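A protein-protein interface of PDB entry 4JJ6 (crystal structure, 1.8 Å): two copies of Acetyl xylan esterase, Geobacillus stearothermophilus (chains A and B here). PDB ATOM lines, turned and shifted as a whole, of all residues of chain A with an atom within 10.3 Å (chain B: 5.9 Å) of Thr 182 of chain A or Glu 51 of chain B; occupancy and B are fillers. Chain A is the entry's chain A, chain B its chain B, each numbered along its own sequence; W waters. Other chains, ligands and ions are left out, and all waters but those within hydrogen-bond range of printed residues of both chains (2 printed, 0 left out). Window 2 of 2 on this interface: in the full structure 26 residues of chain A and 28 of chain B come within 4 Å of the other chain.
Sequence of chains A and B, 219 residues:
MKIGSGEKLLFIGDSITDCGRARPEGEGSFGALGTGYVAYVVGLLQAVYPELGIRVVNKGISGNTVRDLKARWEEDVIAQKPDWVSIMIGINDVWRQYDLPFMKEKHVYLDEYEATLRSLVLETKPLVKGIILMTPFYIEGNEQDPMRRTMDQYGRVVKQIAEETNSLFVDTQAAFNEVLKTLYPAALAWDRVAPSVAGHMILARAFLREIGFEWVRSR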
ATOM      1  N   ILE A 139     -37.771 -20.750 -14.626  1.00  0.00           N
ATOM      2  CA  ILE A 139     -37.147 -21.914 -13.983  1.00  0.00           C
ATOM      3  C   ILE A 139     -38.177 -22.825 -13.428  1.00  0.00           C
ATOM      4  O   ILE A 139     -38.592 -22.736 -12.224  1.00  0.00           O
ATOM      5  CB  ILE A 139     -36.079 -21.470 -12.954  1.00  0.00           C
ATOM      6  CG1 ILE A 139     -35.113 -20.540 -13.624  1.00  0.00           C
ATOM      7  CG2 ILE A 139     -35.394 -22.729 -12.410  1.00  0.00           C
ATOM      8  CD1 ILE A 139     -34.100 -19.896 -12.665  1.00  0.00           C
ATOM      9  N   GLY A 141     -39.943 -26.802 -14.593  1.00  0.00           N
ATOM     10  CA  GLY A 141     -39.786 -27.946 -15.428  1.00  0.00           C
ATOM     11  C   GLY A 141     -41.047 -28.468 -16.062  1.00  0.00           C
ATOM     12  O   GLY A 141     -41.005 -29.127 -17.090  1.00  0.00           O
ATOM     13  N   ALA A 175     -31.291 -24.549 -21.654  1.00  0.00           N
ATOM     14  CA  ALA A 175     -30.192 -24.707 -20.697  1.00  0.00           C
ATOM     15  C   ALA A 175     -30.716 -24.985 -19.327  1.00  0.00           C
ATOM     16  O   ALA A 175     -30.276 -25.922 -18.675  1.00  0.00           O
ATOM     17  CB  ALA A 175     -29.325 -23.486 -20.729  1.00  0.00           C
ATOM     18  N   PHE A 176     -31.759 -24.258 -18.870  1.00  0.00           N
ATOM     19  CA  PHE A 176     -32.293 -24.536 -17.568  1.00  0.00           C
ATOM     20  C   PHE A 176     -32.970 -25.862 -17.548  1.00  0.00           C
ATOM     21  O   PHE A 176     -32.888 -26.623 -16.571  1.00  0.00           O
ATOM     22  CB  PHE A 176     -33.260 -23.410 -17.086  1.00  0.00           C
ATOM     23  CG  PHE A 176     -32.550 -22.222 -16.545  1.00  0.00           C
ATOM     24  CD1 PHE A 176     -31.964 -22.308 -15.280  1.00  0.00           C
ATOM     25  CD2 PHE A 176     -32.488 -21.058 -17.218  1.00  0.00           C
ATOM     26  CE1 PHE A 176     -31.257 -21.248 -14.787  1.00  0.00           C
ATOM     27  CE2 PHE A 176     -31.842 -19.969 -16.688  1.00  0.00           C
ATOM     28  CZ  PHE A 176     -31.233 -20.086 -15.464  1.00  0.00           C
ATOM     29  N   ASN A 177     -33.626 -26.192 -18.659  1.00  0.00           N
ATOM     30  CA  ASN A 177     -34.380 -27.460 -18.698  1.00  0.00           C
ATOM     31  C   ASN A 177     -33.506 -28.691 -18.403  1.00  0.00           C
ATOM     32  O   ASN A 177     -33.919 -29.591 -17.670  1.00  0.00           O
ATOM     33  CB  ASN A 177     -35.035 -27.674 -20.103  1.00  0.00           C
ATOM     34  CG  ASN A 177     -36.245 -26.771 -20.339  1.00  0.00           C
ATOM     35  OD1 ASN A 177     -36.810 -26.216 -19.398  1.00  0.00           O
ATOM     36  ND2 ASN A 177     -36.658 -26.663 -21.603  1.00  0.00           N
ATOM     37  N   GLU A 178     -32.308 -28.629 -18.880  1.00  0.00           N
ATOM     38  CA  GLU A 178     -31.346 -29.720 -18.694  1.00  0.00           C
ATOM     39  C   GLU A 178     -31.069 -29.903 -17.195  1.00  0.00           C
ATOM     40  O   GLU A 178     -31.156 -31.002 -16.639  1.00  0.00           O
ATOM     41  CB  GLU A 178     -30.096 -29.420 -19.500  1.00  0.00           C
ATOM     42  CG  GLU A 178     -28.973 -30.440 -19.377  1.00  0.00           C
ATOM     43  CD  GLU A 178     -29.403 -31.888 -19.720  1.00  0.00           C
ATOM     44  OE1 GLU A 178     -30.366 -32.095 -20.541  1.00  0.00           O
ATOM     45  OE2 GLU A 178     -28.777 -32.833 -19.141  1.00  0.00           O
ATOM     46  N   VAL A 179     -30.824 -28.793 -16.497  1.00  0.00           N
ATOM     47  CA  VAL A 179     -30.548 -28.895 -15.054  1.00  0.00           C
ATOM     48  C   VAL A 179     -31.764 -29.282 -14.251  1.00  0.00           C
ATOM     49  O   VAL A 179     -31.714 -29.989 -13.247  1.00  0.00           O
ATOM     50  CB  VAL A 179     -29.944 -27.562 -14.578  1.00  0.00           C
ATOM     51  CG1 VAL A 179     -29.765 -27.565 -13.067  1.00  0.00           C
ATOM     52  CG2 VAL A 179     -28.651 -27.280 -15.312  1.00  0.00           C
ATOM     53  N   LEU A 180     -32.924 -28.878 -14.740  1.00  0.00           N
ATOM     54  CA  LEU A 180     -34.173 -29.159 -14.128  1.00  0.00           C
ATOM     55  C   LEU A 180     -34.580 -30.607 -14.233  1.00  0.00           C
ATOM     56  O   LEU A 180     -35.493 -31.056 -13.569  1.00  0.00           O
ATOM     57  CB  LEU A 180     -35.301 -28.293 -14.717  1.00  0.00           C
ATOM     58  CG  LEU A 180     -35.316 -26.819 -14.324  1.00  0.00           C
ATOM     59  CD1 LEU A 180     -36.185 -25.976 -15.240  1.00  0.00           C
ATOM     60  CD2 LEU A 180     -35.636 -26.698 -12.866  1.00  0.00           C
ATOM     61  N   LYS A 181     -33.821 -31.375 -14.990  1.00  0.00           N
ATOM     62  CA  LYS A 181     -34.036 -32.813 -14.912  1.00  0.00           C
ATOM     63  C   LYS A 181     -33.581 -33.352 -13.586  1.00  0.00           C
ATOM     64  O   LYS A 181     -33.993 -34.407 -13.141  1.00  0.00           O
ATOM     65  CB  LYS A 181     -33.242 -33.503 -16.019  1.00  0.00           C
ATOM     66  CG  LYS A 181     -33.864 -33.346 -17.391  1.00  0.00           C
ATOM     67  CD  LYS A 181     -32.742 -33.600 -18.377  1.00  0.00           C
ATOM     68  CE  LYS A 181     -33.187 -33.893 -19.801  1.00  0.00           C
ATOM     69  NZ  LYS A 181     -31.991 -33.901 -20.736  1.00  0.00           N
ATOM     70  N   THR A 182     -32.695 -32.619 -12.919  1.00  0.00           N
ATOM     71  CA  THR A 182     -32.151 -33.069 -11.668  1.00  0.00           C
ATOM     72  C   THR A 182     -32.635 -32.243 -10.478  1.00  0.00           C
ATOM     73  O   THR A 182     -32.936 -32.820  -9.451  1.00  0.00           O
ATOM     74  CB  THR A 182     -30.601 -32.979 -11.739  1.00  0.00           C
ATOM     75  OG1 THR A 182     -30.109 -33.792 -12.811  1.00  0.00           O
ATOM     76  CG2 THR A 182     -29.910 -33.298 -10.379  1.00  0.00           C
ATOM     77  N   LEU A 183     -32.673 -30.918 -10.612  1.00  0.00           N
ATOM     78  CA  LEU A 183     -32.975 -30.013  -9.501  1.00  0.00           C
ATOM     79  C   LEU A 183     -34.401 -29.475  -9.566  1.00  0.00           C
ATOM     80  O   LEU A 183     -34.903 -29.140 -10.653  1.00  0.00           O
ATOM     81  CB  LEU A 183     -31.972 -28.845  -9.506  1.00  0.00           C
ATOM     82  CG  LEU A 183     -30.517 -29.197  -9.321  1.00  0.00           C
ATOM     83  CD1 LEU A 183     -29.655 -27.921  -9.389  1.00  0.00           C
ATOM     84  CD2 LEU A 183     -30.399 -29.900  -7.975  1.00  0.00           C
ATOM     85  N   TYR A 184     -35.062 -29.463  -8.428  1.00  0.00           N
ATOM     86  CA  TYR A 184     -36.310 -28.719  -8.287  1.00  0.00           C
ATOM     87  C   TYR A 184     -36.038 -27.216  -8.405  1.00  0.00           C
ATOM     88  O   TYR A 184     -34.974 -26.719  -7.993  1.00  0.00           O
ATOM     89  CB  TYR A 184     -36.920 -29.099  -6.940  1.00  0.00           C
ATOM     90  CG  TYR A 184     -38.316 -28.515  -6.783  1.00  0.00           C
ATOM     91  CD1 TYR A 184     -39.427 -29.137  -7.343  1.00  0.00           C
ATOM     92  CD2 TYR A 184     -38.496 -27.326  -6.085  1.00  0.00           C
ATOM     93  CE1 TYR A 184     -40.703 -28.593  -7.124  1.00  0.00           C
ATOM     94  CE2 TYR A 184     -39.732 -26.737  -5.917  1.00  0.00           C
ATOM     95  CZ  TYR A 184     -40.868 -27.378  -6.472  1.00  0.00           C
ATOM     96  OH  TYR A 184     -42.142 -26.829  -6.316  1.00  0.00           O
ATOM     97  N   PRO A 185     -36.994 -26.397  -8.972  1.00  0.00           N
ATOM     98  CA  PRO A 185     -36.666 -25.034  -9.207  1.00  0.00           C
ATOM     99  C   PRO A 185     -36.053 -24.241  -8.065  1.00  0.00           C
ATOM    100  O   PRO A 185     -35.215 -23.361  -8.253  1.00  0.00           O
ATOM    101  CB  PRO A 185     -37.978 -24.436  -9.600  1.00  0.00           C
ATOM    102  CG  PRO A 185     -38.643 -25.510 -10.408  1.00  0.00           C
ATOM    103  CD  PRO A 185     -38.266 -26.789  -9.680  1.00  0.00           C
ATOM    104  N   ALA A 186     -36.612 -24.451  -6.863  1.00  0.00           N
ATOM    105  CA  ALA A 186     -36.200 -23.742  -5.680  1.00  0.00           C
ATOM    106  C   ALA A 186     -34.725 -23.884  -5.376  1.00  0.00           C
ATOM    107  O   ALA A 186     -34.163 -22.981  -4.787  1.00  0.00           O
ATOM    108  CB  ALA A 186     -37.001 -24.171  -4.464  1.00  0.00           C
ATOM    109  N   ALA A 187     -34.084 -24.968  -5.818  1.00  0.00           N
ATOM    110  CA  ALA A 187     -32.635 -25.104  -5.662  1.00  0.00           C
ATOM    111  C   ALA A 187     -31.817 -24.072  -6.420  1.00  0.00           C
ATOM    112  O   ALA A 187     -30.620 -23.815  -6.116  1.00  0.00           O
ATOM    113  CB  ALA A 187     -32.226 -26.499  -6.034  1.00  0.00           C
ATOM    114  N   LEU A 188     -32.422 -23.507  -7.453  1.00  0.00           N
ATOM    115  CA  LEU A 188     -31.808 -22.522  -8.307  1.00  0.00           C
ATOM    116  C   LEU A 188     -32.396 -21.153  -8.088  1.00  0.00           C
ATOM    117  O   LEU A 188     -31.706 -20.187  -8.177  1.00  0.00           O
ATOM    118  CB  LEU A 188     -32.059 -22.897  -9.784  1.00  0.00           C
ATOM    119  CG  LEU A 188     -31.303 -24.112 -10.360  1.00  0.00           C
ATOM    120  CD1 LEU A 188     -31.822 -24.471 -11.719  1.00  0.00           C
ATOM    121  CD2 LEU A 188     -29.860 -23.773 -10.484  1.00  0.00           C
ATOM    122  N   ILE A 202     -25.248 -20.944 -15.672  1.00  0.00           N
ATOM    123  CA  ILE A 202     -26.024 -21.623 -16.720  1.00  0.00           C
ATOM    124  C   ILE A 202     -26.212 -20.668 -17.856  1.00  0.00           C
ATOM    125  O   ILE A 202     -25.910 -20.992 -18.999  1.00  0.00           O
ATOM    126  CB  ILE A 202     -27.332 -22.157 -16.206  1.00  0.00           C
ATOM    127  CG1 ILE A 202     -27.068 -23.313 -15.270  1.00  0.00           C
ATOM    128  CG2 ILE A 202     -28.282 -22.556 -17.375  1.00  0.00           C
ATOM    129  CD1 ILE A 202     -28.246 -23.696 -14.377  1.00  0.00           C
ATOM    130  N   ARG A 205     -22.759 -19.725 -19.630  1.00  0.00           N
ATOM    131  CA  ARG A 205     -22.245 -20.860 -20.377  1.00  0.00           C
ATOM    132  C   ARG A 205     -23.051 -20.999 -21.661  1.00  0.00           C
ATOM    133  O   ARG A 205     -22.492 -21.240 -22.752  1.00  0.00           O
ATOM    134  CB  ARG A 205     -22.325 -22.072 -19.592  1.00  0.00           C
ATOM    135  CG  ARG A 205     -21.921 -23.364 -20.318  1.00  0.00           C
ATOM    136  CD  ARG A 205     -21.625 -24.404 -19.297  1.00  0.00           C
ATOM    137  NE  ARG A 205     -21.453 -25.730 -19.795  1.00  0.00           N
ATOM    138  CZ  ARG A 205     -22.440 -26.594 -19.995  1.00  0.00           C
ATOM    139  NH1 ARG A 205     -23.722 -26.279 -19.837  1.00  0.00           N
ATOM    140  NH2 ARG A 205     -22.125 -27.810 -20.388  1.00  0.00           N
ATOM    141  N   SER B   5     -20.032 -38.096  -5.933  1.00  0.00           N
ATOM    142  CA  SER B   5     -21.310 -37.611  -5.523  1.00  0.00           C
ATOM    143  C   SER B   5     -21.474 -37.776  -4.040  1.00  0.00           C
ATOM    144  O   SER B   5     -20.960 -38.711  -3.446  1.00  0.00           O
ATOM    145  CB  SER B   5     -22.402 -38.362  -6.321  1.00  0.00           C
ATOM    146  OG  SER B   5     -22.931 -39.399  -5.544  1.00  0.00           O
ATOM    147  N   GLN B  46     -22.479 -27.051 -10.168  1.00  0.00           N
ATOM    148  CA  GLN B  46     -23.912 -27.217 -10.225  1.00  0.00           C
ATOM    149  C   GLN B  46     -24.500 -27.053 -11.659  1.00  0.00           C
ATOM    150  O   GLN B  46     -25.454 -27.727 -12.042  1.00  0.00           O
ATOM    151  CB  GLN B  46     -24.496 -26.241  -9.201  1.00  0.00           C
ATOM    152  CG  GLN B  46     -25.953 -26.335  -8.910  1.00  0.00           C
ATOM    153  CD  GLN B  46     -26.290 -25.666  -7.567  1.00  0.00           C
ATOM    154  OE1 GLN B  46     -25.705 -24.619  -7.169  1.00  0.00           O
ATOM    155  NE2 GLN B  46     -27.168 -26.314  -6.829  1.00  0.00           N
ATOM    156  N   VAL B  48     -23.057 -27.791 -14.441  1.00  0.00           N
ATOM    157  CA  VAL B  48     -22.596 -28.876 -15.338  1.00  0.00           C
ATOM    158  C   VAL B  48     -22.704 -30.268 -14.751  1.00  0.00           C
ATOM    159  O   VAL B  48     -22.867 -31.249 -15.561  1.00  0.00           O
ATOM    160  CB  VAL B  48     -21.201 -28.583 -15.876  1.00  0.00           C
ATOM    161  CG1 VAL B  48     -20.736 -29.644 -16.884  1.00  0.00           C
ATOM    162  CG2 VAL B  48     -21.131 -27.211 -16.525  1.00  0.00           C
ATOM    163  N   TYR B  49     -22.649 -30.392 -13.431  1.00  0.00           N
ATOM    164  CA  TYR B  49     -22.776 -31.645 -12.682  1.00  0.00           C
ATOM    165  C   TYR B  49     -23.805 -31.525 -11.536  1.00  0.00           C
ATOM    166  O   TYR B  49     -23.519 -31.828 -10.367  1.00  0.00           O
ATOM    167  CB  TYR B  49     -21.432 -32.036 -12.042  1.00  0.00           C
ATOM    168  CG  TYR B  49     -20.277 -32.250 -13.062  1.00  0.00           C
ATOM    169  CD1 TYR B  49     -19.803 -33.512 -13.394  1.00  0.00           C
ATOM    170  CD2 TYR B  49     -19.621 -31.191 -13.624  1.00  0.00           C
ATOM    171  CE1 TYR B  49     -18.738 -33.662 -14.284  1.00  0.00           C
ATOM    172  CE2 TYR B  49     -18.569 -31.358 -14.489  1.00  0.00           C
ATOM    173  CZ  TYR B  49     -18.118 -32.595 -14.798  1.00  0.00           C
ATOM    174  OH  TYR B  49     -17.084 -32.724 -15.725  1.00  0.00           O
ATOM    175  N   PRO B  50     -24.994 -31.093 -11.869  1.00  0.00           N
ATOM    176  CA  PRO B  50     -25.980 -30.900 -10.776  1.00  0.00           C
ATOM    177  C   PRO B  50     -26.350 -32.143  -9.967  1.00  0.00           C
ATOM    178  O   PRO B  50     -26.715 -32.102  -8.784  1.00  0.00           O
ATOM    179  CB  PRO B  50     -27.230 -30.436 -11.529  1.00  0.00           C
ATOM    180  CG  PRO B  50     -27.036 -30.798 -12.950  1.00  0.00           C
ATOM    181  CD  PRO B  50     -25.558 -30.854 -13.208  1.00  0.00           C
ATOM    182  N   GLU B  51     -26.192 -33.282 -10.620  1.00  0.00           N
ATOM    183  CA  GLU B  51     -26.560 -34.523 -10.054  1.00  0.00           C
ATOM    184  C   GLU B  51     -25.511 -35.021  -9.107  1.00  0.00           C
ATOM    185  O   GLU B  51     -25.769 -35.927  -8.328  1.00  0.00           O
ATOM    186  CB  GLU B  51     -26.811 -35.517 -11.173  1.00  0.00           C
ATOM    187  CG  GLU B  51     -25.575 -36.183 -11.743  1.00  0.00           C
ATOM    188  CD  GLU B  51     -24.793 -35.379 -12.756  1.00  0.00           C
ATOM    189  OE1 GLU B  51     -25.120 -34.222 -13.042  1.00  0.00           O
ATOM    190  OE2 GLU B  51     -23.776 -35.896 -13.252  1.00  0.00           O
ATOM    191  N   LEU B  52     -24.367 -34.374  -9.050  1.00  0.00           N
ATOM    192  CA  LEU B  52     -23.324 -34.843  -8.119  1.00  0.00           C
ATOM    193  C   LEU B  52     -23.637 -34.589  -6.655  1.00  0.00           C
ATOM    194  O   LEU B  52     -23.233 -35.359  -5.775  1.00  0.00           O
ATOM    195  CB  LEU B  52     -21.933 -34.321  -8.523  1.00  0.00           C
ATOM    196  CG  LEU B  52     -21.233 -35.329  -9.459  1.00  0.00           C
ATOM    197  CD1 LEU B  52     -22.085 -35.879 -10.600  1.00  0.00           C
ATOM    198  CD2 LEU B  52     -19.958 -34.702  -9.986  1.00  0.00           C
ATOM    199  N   GLY B  53     -24.365 -33.545  -6.355  1.00  0.00           N
ATOM    200  CA  GLY B  53     -24.743 -33.372  -4.967  1.00  0.00           C
ATOM    201  C   GLY B  53     -23.553 -33.140  -4.028  1.00  0.00           C
ATOM    202  O   GLY B  53     -23.509 -33.625  -2.919  1.00  0.00           O
ATOM    203  N   ARG B 217     -19.622 -32.054 -21.056  1.00  0.00           N
ATOM    204  CA  ARG B 217     -19.222 -33.380 -20.652  1.00  0.00           C
ATOM    205  C   ARG B 217     -19.331 -34.361 -21.842  1.00  0.00           C
ATOM    206  O   ARG B 217     -20.288 -34.283 -22.607  1.00  0.00           O
ATOM    207  CB  ARG B 217     -20.097 -33.879 -19.526  1.00  0.00           C
ATOM    208  CG  ARG B 217     -19.823 -33.197 -18.205  1.00  0.00           C
ATOM    209  CD  ARG B 217     -20.988 -33.345 -17.308  1.00  0.00           C
ATOM    210  NE  ARG B 217     -21.061 -34.694 -16.802  1.00  0.00           N
ATOM    211  CZ  ARG B 217     -21.878 -35.076 -15.834  1.00  0.00           C
ATOM    212  NH1 ARG B 217     -22.737 -34.249 -15.293  1.00  0.00           N
ATOM    213  NH2 ARG B 217     -21.862 -36.321 -15.389  1.00  0.00           N
HETATM  214  O   HOH W   1     -22.176 -31.018 -20.363  1.00  0.00           O
HETATM  215  O   HOH W   2     -28.225 -22.820  -7.070  1.00  0.00           O
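Among the printed residues, pairs that only touch across the chains: Thr 182 of chain A with Glu 51 of chain B (3.6 Å), Arg 205 of chain A with Val 48 of chain B (3.6 Å), Thr 182 of chain A with Pro 50 of chain B (3.8 Å) and Leu 183 of chain A with Gln 46 of chain B (3.9 Å).
Ala 175 of chain A touches none of the printed residues of chain B.
Of chain B, only Pro 50 and Glu 51 come within 4 Å of Thr 182 of chain A.
Printed residues of chain B within 4 Å of Leu 183 of chain A: Gln 46.
Leu 188 of chain A touches none of the printed residues of chain B.
Printed residues of chain B within 4 Å of Arg 205 of chain A: Val 48 (3.6 Å).
Printed residues of chain A within 4 Å of Gln 46 of chain B: Leu 183.
Printed residues of chain A within 4 Å of Val 48 of chain B: Arg 205.
Of chain A, only Thr 182 (3.6 Å) comes within 4 Å of Glu 51 of chain B.
The nearest printed residue of chain B that does not touch Thr 182 of chain A is Leu 52 of chain B (5.8 Å).
Of the 9 printed residues of chain B, 4 touch a printed residue of chain A.
Hydrophobic or aromatic side chains of chain B that line the printed part of chain A: Val 48.
Printed residues of chain A that touch a printed residue of chain B: Thr 182, Leu 183 and Arg 205.
Hydrophobic or aromatic side chains of chain A within 4 Å of the printed part of chain B: Leu 183.
Among the printed residues, no Asp or Glu carboxylate lies within 4 Å of a Lys or Arg side-chain nitrogen of the other chain.
No position is printed for both chains.
Of the 4 pairs that touch across the chains among the printed residues, none has its exchanged pair printed and touching as well.
The backbone carbonyl oxygen (O) of Val 48 of chain B lies within hydrogen-bond range of the guanidinium group (NH1) of Arg 217 of chain B (3.0 Å).
OE2 of Glu 51 of chain B is in salt-bridge range of NH1 of Arg 217 of chain B, at 2.8 Å.
Water W2 lies within hydrogen-bond range of the backbone carbonyl oxygen of Ala 187 of chain A (2.8 Å) and the side-chain amide oxygen of Gln 46 of chain B (3.1 Å).
Water W1 lies within hydrogen-bond range of N of Arg 217 of chain B and NH2 of Arg 205 of chain A.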
